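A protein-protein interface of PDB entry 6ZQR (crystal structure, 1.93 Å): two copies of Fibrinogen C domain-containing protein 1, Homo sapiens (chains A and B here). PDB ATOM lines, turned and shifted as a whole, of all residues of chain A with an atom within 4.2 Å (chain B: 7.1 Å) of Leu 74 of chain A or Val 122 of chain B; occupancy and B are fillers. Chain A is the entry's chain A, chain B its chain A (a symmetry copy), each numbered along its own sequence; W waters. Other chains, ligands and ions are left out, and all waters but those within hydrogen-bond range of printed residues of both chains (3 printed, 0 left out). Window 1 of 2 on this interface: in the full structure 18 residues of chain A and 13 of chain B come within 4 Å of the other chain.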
ATOM      1  N   VAL A  22      -4.551  -1.968  11.214  1.00  0.00           N
ATOM      2  CA  VAL A  22      -4.153  -1.591   9.832  1.00  0.00           C
ATOM      3  C   VAL A  22      -2.830  -0.832   9.880  1.00  0.00           C
ATOM      4  O   VAL A  22      -2.729   0.142  10.617  1.00  0.00           O
ATOM      5  CB  VAL A  22      -5.267  -0.779   9.155  1.00  0.00           C
ATOM      6  CG1 VAL A  22      -4.876  -0.325   7.759  1.00  0.00           C
ATOM      7  CG2 VAL A  22      -6.558  -1.578   9.119  1.00  0.00           C
ATOM      8  N   GLN A  35      -1.523  -0.745   2.573  1.00  0.00           N
ATOM      9  CA  GLN A  35      -1.984  -1.042   3.941  1.00  0.00           C
ATOM     10  C   GLN A  35      -2.483  -2.480   4.006  1.00  0.00           C
ATOM     11  O   GLN A  35      -3.058  -2.982   3.032  1.00  0.00           O
ATOM     12  CB  GLN A  35      -3.030  -0.015   4.351  1.00  0.00           C
ATOM     13  CG  GLN A  35      -2.426   1.367   4.378  1.00  0.00           C
ATOM     14  CD  GLN A  35      -3.273   2.366   5.117  1.00  0.00           C
ATOM     15  OE1 GLN A  35      -4.478   2.403   4.966  1.00  0.00           O
ATOM     16  NE2 GLN A  35      -2.637   3.176   5.934  1.00  0.00           N
ATOM     17  N   VAL A  36      -2.283  -3.085   5.173  1.00  0.00           N
ATOM     18  CA  VAL A  36      -2.662  -4.483   5.479  1.00  0.00           C
ATOM     19  C   VAL A  36      -3.191  -4.488   6.906  1.00  0.00           C
ATOM     20  O   VAL A  36      -2.889  -3.547   7.679  1.00  0.00           O
ATOM     21  CB  VAL A  36      -1.466  -5.441   5.339  1.00  0.00           C
ATOM     22  CG1 VAL A  36      -0.956  -5.534   3.919  1.00  0.00           C
ATOM     23  CG2 VAL A  36      -0.349  -5.051   6.286  1.00  0.00           C
ATOM     24  N   TYR A  37      -3.956  -5.512   7.224  1.00  0.00           N
ATOM     25  CA  TYR A  37      -4.323  -5.841   8.613  1.00  0.00           C
ATOM     26  C   TYR A  37      -3.249  -6.771   9.180  1.00  0.00           C
ATOM     27  O   TYR A  37      -2.967  -7.830   8.566  1.00  0.00           O
ATOM     28  CB  TYR A  37      -5.706  -6.474   8.683  1.00  0.00           C
ATOM     29  CG  TYR A  37      -6.271  -6.393  10.073  1.00  0.00           C
ATOM     30  CD1 TYR A  37      -5.886  -7.284  11.060  1.00  0.00           C
ATOM     31  CD2 TYR A  37      -7.113  -5.353  10.423  1.00  0.00           C
ATOM     32  CE1 TYR A  37      -6.395  -7.196  12.349  1.00  0.00           C
ATOM     33  CE2 TYR A  37      -7.606  -5.237  11.709  1.00  0.00           C
ATOM     34  CZ  TYR A  37      -7.249  -6.159  12.673  1.00  0.00           C
ATOM     35  OH  TYR A  37      -7.763  -6.030  13.930  1.00  0.00           O
ATOM     36  N   ARG A  52      -9.954 -12.604   4.623  1.00  0.00           N
ATOM     37  CA  ARG A  52     -10.881 -12.782   5.759  1.00  0.00           C
ATOM     38  C   ARG A  52     -12.304 -12.971   5.232  1.00  0.00           C
ATOM     39  O   ARG A  52     -12.761 -12.150   4.386  1.00  0.00           O
ATOM     40  CB  ARG A  52     -10.804 -11.606   6.730  1.00  0.00           C
ATOM     41  CG  ARG A  52     -11.656 -11.788   7.982  1.00  0.00           C
ATOM     42  CD  ARG A  52     -11.651 -10.569   8.865  1.00  0.00           C
ATOM     43  NE  ARG A  52     -10.321 -10.270   9.385  1.00  0.00           N
ATOM     44  CZ  ARG A  52      -9.674  -9.114   9.270  1.00  0.00           C
ATOM     45  NH1 ARG A  52     -10.193  -8.087   8.621  1.00  0.00           N
ATOM     46  NH2 ARG A  52      -8.483  -8.986   9.821  1.00  0.00           N
ATOM     47  N   GLY A  70      -7.435  -7.002  -5.612  1.00  0.00           N
ATOM     48  CA  GLY A  70      -7.981  -7.007  -4.241  1.00  0.00           C
ATOM     49  C   GLY A  70      -9.336  -6.329  -4.152  1.00  0.00           C
ATOM     50  O   GLY A  70      -9.687  -5.551  -5.059  1.00  0.00           O
ATOM     51  N   PHE A  71     -10.098  -6.634  -3.095  1.00  0.00           N
ATOM     52  CA  PHE A  71     -11.466  -6.109  -2.876  1.00  0.00           C
ATOM     53  C   PHE A  71     -11.825  -6.252  -1.393  1.00  0.00           C
ATOM     54  O   PHE A  71     -11.108  -6.902  -0.623  1.00  0.00           O
ATOM     55  CB  PHE A  71     -12.475  -6.827  -3.784  1.00  0.00           C
ATOM     56  CG  PHE A  71     -12.488  -8.333  -3.665  1.00  0.00           C
ATOM     57  CD1 PHE A  71     -13.314  -8.962  -2.740  1.00  0.00           C
ATOM     58  CD2 PHE A  71     -11.679  -9.117  -4.462  1.00  0.00           C
ATOM     59  CE1 PHE A  71     -13.326 -10.345  -2.632  1.00  0.00           C
ATOM     60  CE2 PHE A  71     -11.704 -10.502  -4.365  1.00  0.00           C
ATOM     61  CZ  PHE A  71     -12.530 -11.119  -3.444  1.00  0.00           C
ATOM     62  N   GLY A  72     -12.927  -5.631  -1.008  1.00  0.00           N
ATOM     63  CA  GLY A  72     -13.383  -5.572   0.387  1.00  0.00           C
ATOM     64  C   GLY A  72     -12.598  -4.557   1.196  1.00  0.00           C
ATOM     65  O   GLY A  72     -11.950  -3.658   0.608  1.00  0.00           O
ATOM     66  N   ARG A  73     -12.694  -4.670   2.521  1.00  0.00           N
ATOM     67  CA  ARG A  73     -12.111  -3.693   3.465  1.00  0.00           C
ATOM     68  C   ARG A  73     -11.225  -4.417   4.476  1.00  0.00           C
ATOM     69  O   ARG A  73     -11.582  -5.537   4.913  1.00  0.00           O
ATOM     70  CB  ARG A  73     -13.233  -2.897   4.121  1.00  0.00           C
ATOM     71  CG  ARG A  73     -13.938  -2.001   3.123  1.00  0.00           C
ATOM     72  CD  ARG A  73     -14.908  -1.056   3.753  1.00  0.00           C
ATOM     73  NE  ARG A  73     -15.622  -0.372   2.685  1.00  0.00           N
ATOM     74  CZ  ARG A  73     -16.878   0.037   2.771  1.00  0.00           C
ATOM     75  NH1 ARG A  73     -17.559  -0.172   3.889  1.00  0.00           N
ATOM     76  NH2 ARG A  73     -17.450   0.636   1.736  1.00  0.00           N
ATOM     77  N   LEU A  74     -10.116  -3.771   4.835  1.00  0.00           N
ATOM     78  CA  LEU A  74      -9.043  -4.354   5.677  1.00  0.00           C
ATOM     79  C   LEU A  74      -9.593  -4.699   7.067  1.00  0.00           C
ATOM     80  O   LEU A  74      -9.118  -5.666   7.659  1.00  0.00           O
ATOM     81  CB  LEU A  74      -7.880  -3.364   5.752  1.00  0.00           C
ATOM     82  CG  LEU A  74      -7.096  -3.172   4.449  1.00  0.00           C
ATOM     83  CD1 LEU A  74      -6.018  -2.116   4.615  1.00  0.00           C
ATOM     84  CD2 LEU A  74      -6.476  -4.471   3.975  1.00  0.00           C
ATOM     85  N   THR A  75     -10.574  -3.935   7.542  1.00  0.00           N
ATOM     86  CA  THR A  75     -11.198  -4.076   8.874  1.00  0.00           C
ATOM     87  C   THR A  75     -12.300  -5.135   8.848  1.00  0.00           C
ATOM     88  O   THR A  75     -12.907  -5.356   9.913  1.00  0.00           O
ATOM     89  CB  THR A  75     -11.764  -2.718   9.297  1.00  0.00           C
ATOM     90  OG1 THR A  75     -12.524  -2.255   8.179  1.00  0.00           O
ATOM     91  CG2 THR A  75     -10.669  -1.742   9.665  1.00  0.00           C
ATOM     92  N   GLY A  76     -12.612  -5.707   7.680  1.00  0.00           N
ATOM     93  CA  GLY A  76     -13.709  -6.676   7.542  1.00  0.00           C
ATOM     94  C   GLY A  76     -13.349  -7.783   6.580  1.00  0.00           C
ATOM     95  O   GLY A  76     -12.205  -8.235   6.589  1.00  0.00           O
ATOM     96  N   HIS A  78     -12.242  -9.328   3.197  1.00  0.00           N
ATOM     97  CA  HIS A  78     -11.399  -8.814   2.095  1.00  0.00           C
ATOM     98  C   HIS A  78     -10.513  -9.902   1.527  1.00  0.00           C
ATOM     99  O   HIS A  78     -10.356 -10.960   2.129  1.00  0.00           O
ATOM    100  CB  HIS A  78     -10.564  -7.612   2.526  1.00  0.00           C
ATOM    101  CG  HIS A  78      -9.453  -7.924   3.473  1.00  0.00           C
ATOM    102  ND1 HIS A  78      -9.671  -8.137   4.825  1.00  0.00           N
ATOM    103  CD2 HIS A  78      -8.121  -8.038   3.277  1.00  0.00           C
ATOM    104  CE1 HIS A  78      -8.528  -8.384   5.417  1.00  0.00           C
ATOM    105  NE2 HIS A  78      -7.545  -8.320   4.493  1.00  0.00           N
ATOM    106  N   TRP A  79      -9.987  -9.586   0.354  1.00  0.00           N
ATOM    107  CA  TRP A  79      -8.935 -10.326  -0.361  1.00  0.00           C
ATOM    108  C   TRP A  79      -7.920  -9.262  -0.770  1.00  0.00           C
ATOM    109  O   TRP A  79      -8.354  -8.281  -1.414  1.00  0.00           O
ATOM    110  CB  TRP A  79      -9.522 -11.039  -1.573  1.00  0.00           C
ATOM    111  CG  TRP A  79      -8.487 -11.687  -2.424  1.00  0.00           C
ATOM    112  CD1 TRP A  79      -7.924 -11.202  -3.571  1.00  0.00           C
ATOM    113  CD2 TRP A  79      -7.873 -12.959  -2.177  1.00  0.00           C
ATOM    114  NE1 TRP A  79      -7.006 -12.094  -4.052  1.00  0.00           N
ATOM    115  CE2 TRP A  79      -6.969 -13.193  -3.238  1.00  0.00           C
ATOM    116  CE3 TRP A  79      -8.042 -13.938  -1.196  1.00  0.00           C
ATOM    117  CZ2 TRP A  79      -6.214 -14.363  -3.327  1.00  0.00           C
ATOM    118  CZ3 TRP A  79      -7.300 -15.103  -1.287  1.00  0.00           C
ATOM    119  CH2 TRP A  79      -6.392 -15.306  -2.337  1.00  0.00           C
ATOM    120  N   LEU A  80      -6.679  -9.396  -0.322  1.00  0.00           N
ATOM    121  CA  LEU A  80      -5.664  -8.319  -0.410  1.00  0.00           C
ATOM    122  C   LEU A  80      -5.260  -8.116  -1.871  1.00  0.00           C
ATOM    123  O   LEU A  80      -4.801  -7.008  -2.213  1.00  0.00           O
ATOM    124  CB  LEU A  80      -4.458  -8.700   0.453  1.00  0.00           C
ATOM    125  CG  LEU A  80      -3.360  -7.648   0.582  1.00  0.00           C
ATOM    126  CD1 LEU A  80      -3.892  -6.359   1.201  1.00  0.00           C
ATOM    127  CD2 LEU A  80      -2.211  -8.183   1.417  1.00  0.00           C
ATOM    128  N   ARG A  84      -0.365  -8.142  -4.551  1.00  0.00           N
ATOM    129  CA  ARG A  84       0.214  -7.816  -3.223  1.00  0.00           C
ATOM    130  C   ARG A  84       0.764  -9.080  -2.556  1.00  0.00           C
ATOM    131  O   ARG A  84       1.839  -8.994  -1.947  1.00  0.00           O
ATOM    132  CB  ARG A  84      -0.819  -7.085  -2.376  1.00  0.00           C
ATOM    133  CG  ARG A  84      -1.242  -5.772  -3.025  1.00  0.00           C
ATOM    134  CD  ARG A  84      -2.042  -4.903  -2.106  1.00  0.00           C
ATOM    135  NE  ARG A  84      -2.479  -3.689  -2.795  1.00  0.00           N
ATOM    136  CZ  ARG A  84      -3.654  -3.510  -3.371  1.00  0.00           C
ATOM    137  NH1 ARG A  84      -4.566  -4.471  -3.381  1.00  0.00           N
ATOM    138  NH2 ARG A  84      -3.915  -2.354  -3.958  1.00  0.00           N
ATOM    139  N   HIS B  86      -7.518  10.093  -1.360  1.00  0.00           N
ATOM    140  CA  HIS B  86      -7.274   8.783  -0.695  1.00  0.00           C
ATOM    141  C   HIS B  86      -5.824   8.711  -0.182  1.00  0.00           C
ATOM    142  O   HIS B  86      -5.642   8.411   1.020  1.00  0.00           O
ATOM    143  CB  HIS B  86      -7.646   7.609  -1.605  1.00  0.00           C
ATOM    144  CG  HIS B  86      -7.242   6.297  -1.028  1.00  0.00           C
ATOM    145  ND1 HIS B  86      -6.076   5.669  -1.405  1.00  0.00           N
ATOM    146  CD2 HIS B  86      -7.816   5.522  -0.075  1.00  0.00           C
ATOM    147  CE1 HIS B  86      -5.931   4.561  -0.705  1.00  0.00           C
ATOM    148  NE2 HIS B  86      -6.997   4.436   0.118  1.00  0.00           N
ATOM    149  N   GLY B 118     -12.171   6.223   1.163  1.00  0.00           N
ATOM    150  CA  GLY B 118     -11.741   4.811   1.034  1.00  0.00           C
ATOM    151  C   GLY B 118     -10.724   4.399   2.091  1.00  0.00           C
ATOM    152  O   GLY B 118      -9.758   3.708   1.733  1.00  0.00           O
ATOM    153  N   LEU B 119     -10.921   4.791   3.354  1.00  0.00           N
ATOM    154  CA  LEU B 119      -9.884   4.651   4.413  1.00  0.00           C
ATOM    155  C   LEU B 119      -9.430   3.189   4.567  1.00  0.00           C
ATOM    156  O   LEU B 119      -8.219   2.985   4.779  1.00  0.00           O
ATOM    157  CB  LEU B 119     -10.394   5.221   5.743  1.00  0.00           C
ATOM    158  CG  LEU B 119     -10.417   6.751   5.828  1.00  0.00           C
ATOM    159  CD1 LEU B 119     -10.640   7.215   7.258  1.00  0.00           C
ATOM    160  CD2 LEU B 119      -9.133   7.354   5.276  1.00  0.00           C
ATOM    161  N   PHE B 120     -10.321   2.204   4.519  1.00  0.00           N
ATOM    162  CA  PHE B 120      -9.895   0.790   4.751  1.00  0.00           C
ATOM    163  C   PHE B 120     -10.134  -0.065   3.507  1.00  0.00           C
ATOM    164  O   PHE B 120      -9.969  -1.304   3.577  1.00  0.00           O
ATOM    165  CB  PHE B 120     -10.589   0.263   6.004  1.00  0.00           C
ATOM    166  CG  PHE B 120     -10.261   1.086   7.219  1.00  0.00           C
ATOM    167  CD1 PHE B 120      -8.969   1.117   7.721  1.00  0.00           C
ATOM    168  CD2 PHE B 120     -11.226   1.860   7.840  1.00  0.00           C
ATOM    169  CE1 PHE B 120      -8.660   1.887   8.833  1.00  0.00           C
ATOM    170  CE2 PHE B 120     -10.913   2.634   8.948  1.00  0.00           C
ATOM    171  CZ  PHE B 120      -9.634   2.646   9.440  1.00  0.00           C
ATOM    172  N   SER B 121     -10.455   0.577   2.383  1.00  0.00           N
ATOM    173  CA  SER B 121     -10.747  -0.101   1.100  1.00  0.00           C
ATOM    174  C   SER B 121      -9.452  -0.723   0.565  1.00  0.00           C
ATOM    175  O   SER B 121      -8.451  -0.001   0.446  1.00  0.00           O
ATOM    176  CB  SER B 121     -11.356   0.854   0.115  1.00  0.00           C
ATOM    177  OG  SER B 121     -12.425   1.579   0.706  1.00  0.00           O
ATOM    178  N   VAL B 122      -9.477  -2.009   0.222  1.00  0.00           N
ATOM    179  CA  VAL B 122      -8.319  -2.683  -0.434  1.00  0.00           C
ATOM    180  C   VAL B 122      -8.140  -2.077  -1.827  1.00  0.00           C
ATOM    181  O   VAL B 122      -6.998  -1.807  -2.226  1.00  0.00           O
ATOM    182  CB  VAL B 122      -8.496  -4.210  -0.493  1.00  0.00           C
ATOM    183  CG1 VAL B 122      -7.407  -4.865  -1.325  1.00  0.00           C
ATOM    184  CG2 VAL B 122      -8.553  -4.816   0.898  1.00  0.00           C
ATOM    185  N   ASP B 123      -9.226  -1.926  -2.565  1.00  0.00           N
ATOM    186  CA  ASP B 123      -9.237  -1.232  -3.878  1.00  0.00           C
ATOM    187  C   ASP B 123     -10.155  -0.023  -3.712  1.00  0.00           C
ATOM    188  O   ASP B 123     -11.359  -0.138  -3.920  1.00  0.00           O
ATOM    189  CB  ASP B 123      -9.687  -2.186  -4.987  1.00  0.00           C
ATOM    190  CG  ASP B 123      -9.731  -1.568  -6.377  1.00  0.00           C
ATOM    191  OD1 ASP B 123      -9.755  -0.308  -6.482  1.00  0.00           O
ATOM    192  OD2 ASP B 123      -9.751  -2.352  -7.347  1.00  0.00           O
ATOM    193  N   PRO B 124      -9.632   1.148  -3.287  1.00  0.00           N
ATOM    194  CA  PRO B 124     -10.504   2.295  -3.007  1.00  0.00           C
ATOM    195  C   PRO B 124     -11.352   2.715  -4.217  1.00  0.00           C
ATOM    196  O   PRO B 124     -12.480   3.132  -4.018  1.00  0.00           O
ATOM    197  CB  PRO B 124      -9.533   3.384  -2.525  1.00  0.00           C
ATOM    198  CG  PRO B 124      -8.189   2.962  -3.077  1.00  0.00           C
ATOM    199  CD  PRO B 124      -8.207   1.447  -3.066  1.00  0.00           C
ATOM    200  N   GLU B 125     -10.837   2.562  -5.437  1.00  0.00           N
ATOM    201  CA  GLU B 125     -11.596   2.912  -6.660  1.00  0.00           C
ATOM    202  C   GLU B 125     -12.818   1.994  -6.800  1.00  0.00           C
ATOM    203  O   GLU B 125     -13.946   2.520  -6.937  1.00  0.00           O
ATOM    204  CB  GLU B 125     -10.708   2.871  -7.904  1.00  0.00           C
ATOM    205  CG  GLU B 125     -11.439   3.390  -9.123  1.00  0.00           C
ATOM    206  CD  GLU B 125     -10.751   3.238 -10.465  1.00  0.00           C
ATOM    207  OE1 GLU B 125      -9.654   2.680 -10.508  1.00  0.00           O
ATOM    208  OE2 GLU B 125     -11.319   3.697 -11.460  1.00  0.00           O
ATOM    209  N   ASP B 127     -14.246   0.126  -4.558  1.00  0.00           N
ATOM    210  CA  ASP B 127     -15.079   0.349  -3.350  1.00  0.00           C
ATOM    211  C   ASP B 127     -15.802   1.707  -3.441  1.00  0.00           C
ATOM    212  O   ASP B 127     -16.649   1.971  -2.585  1.00  0.00           O
ATOM    213  CB  ASP B 127     -14.242   0.241  -2.075  1.00  0.00           C
ATOM    214  CG  ASP B 127     -15.056  -0.159  -0.852  1.00  0.00           C
ATOM    215  OD1 ASP B 127     -16.144  -0.757  -1.042  1.00  0.00           O
ATOM    216  OD2 ASP B 127     -14.620   0.158   0.277  1.00  0.00           O
HETATM  217  O   HOH W   1     -10.652  -4.698  -7.407  1.00  0.00           O
HETATM  218  O   HOH W   2      -6.202  -2.532  -5.168  1.00  0.00           O
HETATM  219  O   HOH W   3     -11.899  -2.460  -1.895  1.00  0.00           O
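Of the 16 printed residues of chain A, 12 touch a printed residue of chain B. Printed residues of chain A that touch a printed residue of chain B: Val 22, Gln 35, Gly 70, Phe 71, Gly 72, Arg 73, Leu 74, Thr 75, His 78, Trp 79, Leu 80 and Arg 84. Hydrophobic or aromatic side chains of chain A that line the printed part of chain B: Val 22, Leu 74 and His 78. Hydrophobic or aromatic side chains of chain B that line the printed part of chain A: Phe 120 and Val 122. Among the printed residues, 16 pairs touch across the chains.
The guanidinium group (NH1) of Arg 52 of chain A is in hydrogen-bond range of the backbone carbonyl oxygen (O) of Leu 74 of chain A, 2.8 Å away. OD1 of Asp 123 of chain B lies close to N of Glu 125 of chain B, 3.2 Å away. O of Arg 73 of chain A lies within hydrogen-bond range of ND1 of His 78 of chain A, 3.2 Å away. The backbone carbonyl oxygen (O) of Leu 80 of chain A sits at hydrogen-bond distance from the guanidinium group (NH1) of Arg 84 of chain A (2.8 Å). The backbone NH (N) of Arg 52 of chain A is in hydrogen-bond range of the backbone carbonyl oxygen (O) of His 78 of chain A (3.0 Å). The side-chain hydroxyl (OG) of Ser 121 of chain B sits at hydrogen-bond distance from the side-chain carboxylate (OD2) of Asp 127 of chain B, at 2.6 Å.
Printed residues of chain B within 4 Å of Arg 73 of chain A: Phe 120 (3.2 Å) and Asp 127 (2.7 Å). Of chain B, only Phe 120 and Val 122 come within 4 Å of Leu 74 of chain A. Printed residues of chain A within 4 Å of Phe 120 of chain B: Val 22 (3.9 Å), Arg 73 (3.2 Å), Leu 74 (2.8 Å) and Thr 75 (3.8 Å). Pro 124 of chain B touches none of the printed residues of chain A. The nearest residue of chain B that does not touch Leu 74 of chain A is Ser 121 of chain B (5.0 Å). The nearest printed residue of chain A that does not touch Val 122 of chain B is Arg 73 of chain A (4.5 Å).
The guanidinium group of Arg 73 of chain A lies within salt-bridge range of the side-chain carboxylate of Asp 127 of chain B, 2.7 Å away. The backbone NH (N) of Val 122 of chain B lies within hydrogen-bond range of the backbone carbonyl oxygen (O) of Gly 72 of chain A (3.0 Å). The backbone NH of Leu 74 of chain A is in hydrogen-bond range of the backbone carbonyl oxygen of Phe 120 of chain B (2.8 Å).
Water W1 lies within hydrogen-bond range of OD2 of Asp 123 of chain B and O of Gly 70 of chain A. Water W2 bridges NH2 of Arg 84 of chain A and O of Val 122 of chain B. Water W3 lies within hydrogen-bond range of O of Gly 72 of chain A (2.8 Å), N of Asp 123 of chain B (2.8 Å) and N of Val 122 of chain B (3.2 Å).
Among the printed residues, pairs that only touch across the chains: Val 22 of chain A with Phe 120 of chain B (3.9 Å), Gln 35 of chain A with Leu 119 of chain B (3.8 Å), Gly 70 of chain A with Val 122 of chain B (3.7 Å), Gly 70 of chain A with Asp 123 of chain B (3.4 Å), Phe 71 of chain A with Val 122 of chain B (3.6 Å), Gly 72 of chain A with Ser 121 of chain B (3.8 Å), Arg 73 of chain A with Phe 120 of chain B (3.2 Å), Leu 74 of chain A with Val 122 of chain B (3.7 Å), Thr 75 of chain A with Phe 120 of chain B (3.8 Å), His 78 of chain A with Val 122 of chain B (3.8 Å), Trp 79 of chain A with Val 122 of chain B (3.5 Å), Leu 80 of chain A with Val 122 of chain B (3.5 Å) and Arg 84 of chain A with Val 122 of chain B (3.5 Å).
No position is printed for both chains. Of the 16 pairs that touch across the chains among the printed residues, none has its exchanged pair printed and touching as well.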
